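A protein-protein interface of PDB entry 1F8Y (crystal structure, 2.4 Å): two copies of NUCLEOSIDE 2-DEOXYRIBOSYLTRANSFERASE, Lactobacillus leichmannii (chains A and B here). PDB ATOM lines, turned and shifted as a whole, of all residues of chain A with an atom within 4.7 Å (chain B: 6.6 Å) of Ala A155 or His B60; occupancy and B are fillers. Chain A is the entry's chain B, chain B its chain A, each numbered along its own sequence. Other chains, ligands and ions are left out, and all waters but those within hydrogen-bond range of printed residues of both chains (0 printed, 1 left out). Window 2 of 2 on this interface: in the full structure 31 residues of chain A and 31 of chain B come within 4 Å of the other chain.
Among the printed residues, merely in contact across the chains: Gly A154 with His B60, Ala A155 with Leu B59, Ala A155 with His B60 and Tyr A157 with Val B52.
Of the 8 printed residues of chain B, 3 touch a printed residue of chain A. Hydrophobic or aromatic side chains of chain B that line the printed part of chain A: Val B52, Leu B59 and His B60. Of the 9 printed residues of chain A, 4 touch a printed residue of chain B. Printed residues of chain A that touch a printed residue of chain B: Gly A154, Ala A155, Val A156 and Tyr A157. Among the printed residues, no Asp or Glu carboxylate lies within 4 Å of a Lys or Arg side-chain nitrogen of the other chain.
O of Gly A119 sits at hydrogen-bond distance from N of Ala A155. N of Ile A122 lies within hydrogen-bond range of O of Ala A155 (3.0 Å). The backbone carbonyl oxygen of Ile A122 sits at hydrogen-bond distance from the backbone NH of Tyr A157 (3.0 Å).
The backbone carbonyl oxygen (O) of Leu B59 is in hydrogen-bond range of the backbone NH (N) of Val A156 (3.1 Å).
Printed residues of chain B within 4 Å of Ala A155: Leu B59 (3.2 Å) and His B60 (3.4 Å). Of chain A, only Gly A154 (3.7 Å) and Ala A155 (3.4 Å) come within 4 Å of His B60. Of the printed residues of chain A, Leu B59 touches Ala A155 (3.2 Å) and Val A156 (3.1 Å). Of the printed residues of chain A, Val B52 touches Tyr A157 (3.1 Å). Of the printed residues of chain B, Gly A154 touches His B60.
No position is printed for both chains.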
ATOM      1  N   GLY A 119      -2.494  -2.076 -16.320  1.00  0.00           N
ATOM      2  CA  GLY A 119      -2.409  -2.949 -17.470  1.00  0.00           C
ATOM      3  C   GLY A 119      -3.796  -3.374 -17.919  1.00  0.00           C
ATOM      4  O   GLY A 119      -4.020  -3.588 -19.112  1.00  0.00           O
ATOM      5  N   LYS A 120      -4.713  -3.525 -16.961  1.00  0.00           N
ATOM      6  CA  LYS A 120      -6.099  -3.920 -17.242  1.00  0.00           C
ATOM      7  C   LYS A 120      -6.738  -2.910 -18.184  1.00  0.00           C
ATOM      8  O   LYS A 120      -6.350  -1.749 -18.208  1.00  0.00           O
ATOM      9  CB  LYS A 120      -6.907  -3.990 -15.949  1.00  0.00           C
ATOM     10  CG  LYS A 120      -6.554  -5.164 -15.052  1.00  0.00           C
ATOM     11  CD  LYS A 120      -7.366  -5.112 -13.766  1.00  0.00           C
ATOM     12  CE  LYS A 120      -7.081  -6.315 -12.890  1.00  0.00           C
ATOM     13  NZ  LYS A 120      -7.757  -6.191 -11.577  1.00  0.00           N
ATOM     14  N   PRO A 121      -7.736  -3.336 -18.967  1.00  0.00           N
ATOM     15  CA  PRO A 121      -8.351  -2.371 -19.885  1.00  0.00           C
ATOM     16  C   PRO A 121      -9.156  -1.246 -19.248  1.00  0.00           C
ATOM     17  O   PRO A 121      -9.905  -1.466 -18.289  1.00  0.00           O
ATOM     18  CB  PRO A 121      -9.208  -3.257 -20.792  1.00  0.00           C
ATOM     19  CG  PRO A 121      -9.581  -4.393 -19.904  1.00  0.00           C
ATOM     20  CD  PRO A 121      -8.285  -4.688 -19.178  1.00  0.00           C
ATOM     21  N   ILE A 122      -8.974  -0.038 -19.782  1.00  0.00           N
ATOM     22  CA  ILE A 122      -9.689   1.145 -19.319  1.00  0.00           C
ATOM     23  C   ILE A 122     -10.505   1.694 -20.480  1.00  0.00           C
ATOM     24  O   ILE A 122     -10.205   1.428 -21.645  1.00  0.00           O
ATOM     25  CB  ILE A 122      -8.746   2.251 -18.780  1.00  0.00           C
ATOM     26  CG1 ILE A 122      -7.841   2.793 -19.898  1.00  0.00           C
ATOM     27  CG2 ILE A 122      -7.935   1.716 -17.605  1.00  0.00           C
ATOM     28  CD1 ILE A 122      -7.100   4.089 -19.533  1.00  0.00           C
ATOM     29  N   TYR A 152      -0.599   5.135 -21.993  1.00  0.00           N
ATOM     30  CA  TYR A 152      -0.823   4.124 -20.965  1.00  0.00           C
ATOM     31  C   TYR A 152      -0.305   2.781 -21.465  1.00  0.00           C
ATOM     32  O   TYR A 152      -0.731   2.315 -22.513  1.00  0.00           O
ATOM     33  CB  TYR A 152      -2.325   4.013 -20.702  1.00  0.00           C
ATOM     34  CG  TYR A 152      -2.785   2.827 -19.878  1.00  0.00           C
ATOM     35  CD1 TYR A 152      -2.246   2.571 -18.619  1.00  0.00           C
ATOM     36  CD2 TYR A 152      -3.829   2.009 -20.328  1.00  0.00           C
ATOM     37  CE1 TYR A 152      -2.738   1.544 -17.825  1.00  0.00           C
ATOM     38  CE2 TYR A 152      -4.335   0.977 -19.535  1.00  0.00           C
ATOM     39  CZ  TYR A 152      -3.785   0.756 -18.284  1.00  0.00           C
ATOM     40  OH  TYR A 152      -4.300  -0.222 -17.469  1.00  0.00           O
ATOM     41  N   GLY A 154      -1.017  -0.247 -21.454  1.00  0.00           N
ATOM     42  CA  GLY A 154      -2.088  -1.157 -21.102  1.00  0.00           C
ATOM     43  C   GLY A 154      -3.154  -1.207 -22.177  1.00  0.00           C
ATOM     44  O   GLY A 154      -3.016  -0.573 -23.224  1.00  0.00           O
ATOM     45  N   ALA A 155      -4.211  -1.970 -21.934  1.00  0.00           N
ATOM     46  CA  ALA A 155      -5.278  -2.107 -22.915  1.00  0.00           C
ATOM     47  C   ALA A 155      -6.383  -1.077 -22.731  1.00  0.00           C
ATOM     48  O   ALA A 155      -6.606  -0.584 -21.620  1.00  0.00           O
ATOM     49  CB  ALA A 155      -5.858  -3.499 -22.852  1.00  0.00           C
ATOM     50  N   VAL A 156      -7.049  -0.728 -23.830  1.00  0.00           N
ATOM     51  CA  VAL A 156      -8.164   0.213 -23.774  1.00  0.00           C
ATOM     52  C   VAL A 156      -9.323  -0.382 -24.589  1.00  0.00           C
ATOM     53  O   VAL A 156      -9.146  -0.766 -25.753  1.00  0.00           O
ATOM     54  CB  VAL A 156      -7.768   1.666 -24.233  1.00  0.00           C
ATOM     55  CG1 VAL A 156      -6.272   1.796 -24.424  1.00  0.00           C
ATOM     56  CG2 VAL A 156      -8.513   2.088 -25.488  1.00  0.00           C
ATOM     57  N   TYR A 157     -10.472  -0.551 -23.929  1.00  0.00           N
ATOM     58  CA  TYR A 157     -11.661  -1.111 -24.566  1.00  0.00           C
ATOM     59  C   TYR A 157     -12.558  -0.012 -25.122  1.00  0.00           C
ATOM     60  O   TYR A 157     -13.486  -0.365 -25.877  1.00  0.00           O
ATOM     61  CB  TYR A 157     -12.452  -1.992 -23.584  1.00  0.00           C
ATOM     62  CG  TYR A 157     -13.172  -1.244 -22.483  1.00  0.00           C
ATOM     63  CD1 TYR A 157     -14.463  -0.742 -22.685  1.00  0.00           C
ATOM     64  CD2 TYR A 157     -12.572  -1.030 -21.247  1.00  0.00           C
ATOM     65  CE1 TYR A 157     -15.130  -0.045 -21.696  1.00  0.00           C
ATOM     66  CE2 TYR A 157     -13.239  -0.336 -20.243  1.00  0.00           C
ATOM     67  CZ  TYR A 157     -14.519   0.157 -20.487  1.00  0.00           C
ATOM     68  OH  TYR A 157     -15.190   0.876 -19.529  1.00  0.00           O
ATOM     69  OXT TYR A 157     -12.343   1.175 -24.767  1.00  0.00           O
ATOM     70  N   VAL B  52     -13.767  -3.267 -30.707  1.00  0.00           N
ATOM     71  CA  VAL B  52     -12.751  -4.027 -29.988  1.00  0.00           C
ATOM     72  C   VAL B  52     -13.296  -5.240 -29.270  1.00  0.00           C
ATOM     73  O   VAL B  52     -12.538  -6.150 -28.946  1.00  0.00           O
ATOM     74  CB  VAL B  52     -11.994  -3.183 -28.947  1.00  0.00           C
ATOM     75  CG1 VAL B  52     -11.113  -2.171 -29.634  1.00  0.00           C
ATOM     76  CG2 VAL B  52     -12.968  -2.507 -28.007  1.00  0.00           C
ATOM     77  N   PRO B  56     -10.725  -8.367 -30.219  1.00  0.00           N
ATOM     78  CA  PRO B  56      -9.871  -8.053 -29.069  1.00  0.00           C
ATOM     79  C   PRO B  56      -8.437  -7.686 -29.393  1.00  0.00           C
ATOM     80  O   PRO B  56      -7.757  -7.095 -28.558  1.00  0.00           O
ATOM     81  CB  PRO B  56      -9.945  -9.320 -28.226  1.00  0.00           C
ATOM     82  CG  PRO B  56     -11.333  -9.814 -28.506  1.00  0.00           C
ATOM     83  CD  PRO B  56     -11.420  -9.649 -30.008  1.00  0.00           C
ATOM     84  N   GLU B  57      -7.975  -8.016 -30.597  1.00  0.00           N
ATOM     85  CA  GLU B  57      -6.606  -7.697 -30.986  1.00  0.00           C
ATOM     86  C   GLU B  57      -6.376  -6.186 -30.998  1.00  0.00           C
ATOM     87  O   GLU B  57      -5.247  -5.716 -30.879  1.00  0.00           O
ATOM     88  CB  GLU B  57      -6.255  -8.299 -32.354  1.00  0.00           C
ATOM     89  CG  GLU B  57      -7.032  -7.753 -33.548  1.00  0.00           C
ATOM     90  CD  GLU B  57      -8.187  -8.652 -33.982  1.00  0.00           C
ATOM     91  OE1 GLU B  57      -8.697  -9.425 -33.143  1.00  0.00           O
ATOM     92  OE2 GLU B  57      -8.594  -8.576 -35.165  1.00  0.00           O
ATOM     93  N   TYR B  58      -7.458  -5.424 -31.101  1.00  0.00           N
ATOM     94  CA  TYR B  58      -7.359  -3.975 -31.121  1.00  0.00           C
ATOM     95  C   TYR B  58      -7.246  -3.330 -29.745  1.00  0.00           C
ATOM     96  O   TYR B  58      -7.044  -2.131 -29.642  1.00  0.00           O
ATOM     97  CB  TYR B  58      -8.499  -3.373 -31.935  1.00  0.00           C
ATOM     98  CG  TYR B  58      -8.329  -3.608 -33.419  1.00  0.00           C
ATOM     99  CD1 TYR B  58      -7.759  -2.631 -34.241  1.00  0.00           C
ATOM    100  CD2 TYR B  58      -8.679  -4.831 -33.997  1.00  0.00           C
ATOM    101  CE1 TYR B  58      -7.537  -2.867 -35.595  1.00  0.00           C
ATOM    102  CE2 TYR B  58      -8.459  -5.077 -35.356  1.00  0.00           C
ATOM    103  CZ  TYR B  58      -7.885  -4.092 -36.145  1.00  0.00           C
ATOM    104  OH  TYR B  58      -7.623  -4.341 -37.478  1.00  0.00           O
ATOM    105  N   LEU B  59      -7.308  -4.135 -28.695  1.00  0.00           N
ATOM    106  CA  LEU B  59      -7.185  -3.647 -27.318  1.00  0.00           C
ATOM    107  C   LEU B  59      -5.839  -2.989 -27.083  1.00  0.00           C
ATOM    108  O   LEU B  59      -5.630  -2.317 -26.067  1.00  0.00           O
ATOM    109  CB  LEU B  59      -7.302  -4.805 -26.324  1.00  0.00           C
ATOM    110  CG  LEU B  59      -8.652  -5.440 -26.023  1.00  0.00           C
ATOM    111  CD1 LEU B  59      -8.422  -6.676 -25.184  1.00  0.00           C
ATOM    112  CD2 LEU B  59      -9.546  -4.446 -25.287  1.00  0.00           C
ATOM    113  N   HIS B  60      -4.886  -3.319 -27.951  1.00  0.00           N
ATOM    114  CA  HIS B  60      -3.530  -2.790 -27.866  1.00  0.00           C
ATOM    115  C   HIS B  60      -3.162  -2.255 -29.240  1.00  0.00           C
ATOM    116  O   HIS B  60      -2.424  -2.889 -29.999  1.00  0.00           O
ATOM    117  CB  HIS B  60      -2.552  -3.892 -27.440  1.00  0.00           C
ATOM    118  CG  HIS B  60      -2.604  -4.221 -25.980  1.00  0.00           C
ATOM    119  ND1 HIS B  60      -3.460  -5.169 -25.457  1.00  0.00           N
ATOM    120  CD2 HIS B  60      -1.892  -3.741 -24.932  1.00  0.00           C
ATOM    121  CE1 HIS B  60      -3.270  -5.260 -24.152  1.00  0.00           C
ATOM    122  NE2 HIS B  60      -2.324  -4.405 -23.808  1.00  0.00           N
ATOM    123  N   ASP B  61      -3.761  -1.126 -29.584  1.00  0.00           N
ATOM    124  CA  ASP B  61      -3.527  -0.470 -30.857  1.00  0.00           C
ATOM    125  C   ASP B  61      -3.812   1.008 -30.623  1.00  0.00           C
ATOM    126  O   ASP B  61      -4.955   1.432 -30.648  1.00  0.00           O
ATOM    127  CB  ASP B  61      -4.466  -1.039 -31.926  1.00  0.00           C
ATOM    128  CG  ASP B  61      -4.215  -0.446 -33.301  1.00  0.00           C
ATOM    129  OD1 ASP B  61      -3.605   0.636 -33.397  1.00  0.00           O
ATOM    130  OD2 ASP B  61      -4.636  -1.058 -34.301  1.00  0.00           O
ATOM    131  N   LYS B  62      -2.755   1.779 -30.394  1.00  0.00           N
ATOM    132  CA  LYS B  62      -2.879   3.208 -30.141  1.00  0.00           C
ATOM    133  C   LYS B  62      -3.552   3.949 -31.289  1.00  0.00           C
ATOM    134  O   LYS B  62      -4.317   4.879 -31.062  1.00  0.00           O
ATOM    135  CB  LYS B  62      -1.512   3.822 -29.840  1.00  0.00           C
ATOM    136  CG  LYS B  62      -0.839   3.252 -28.605  1.00  0.00           C
ATOM    137  CD  LYS B  62       0.515   3.900 -28.380  1.00  0.00           C
ATOM    138  CE  LYS B  62       1.258   3.276 -27.216  1.00  0.00           C
ATOM    139  NZ  LYS B  62       1.471   1.826 -27.426  1.00  0.00           N
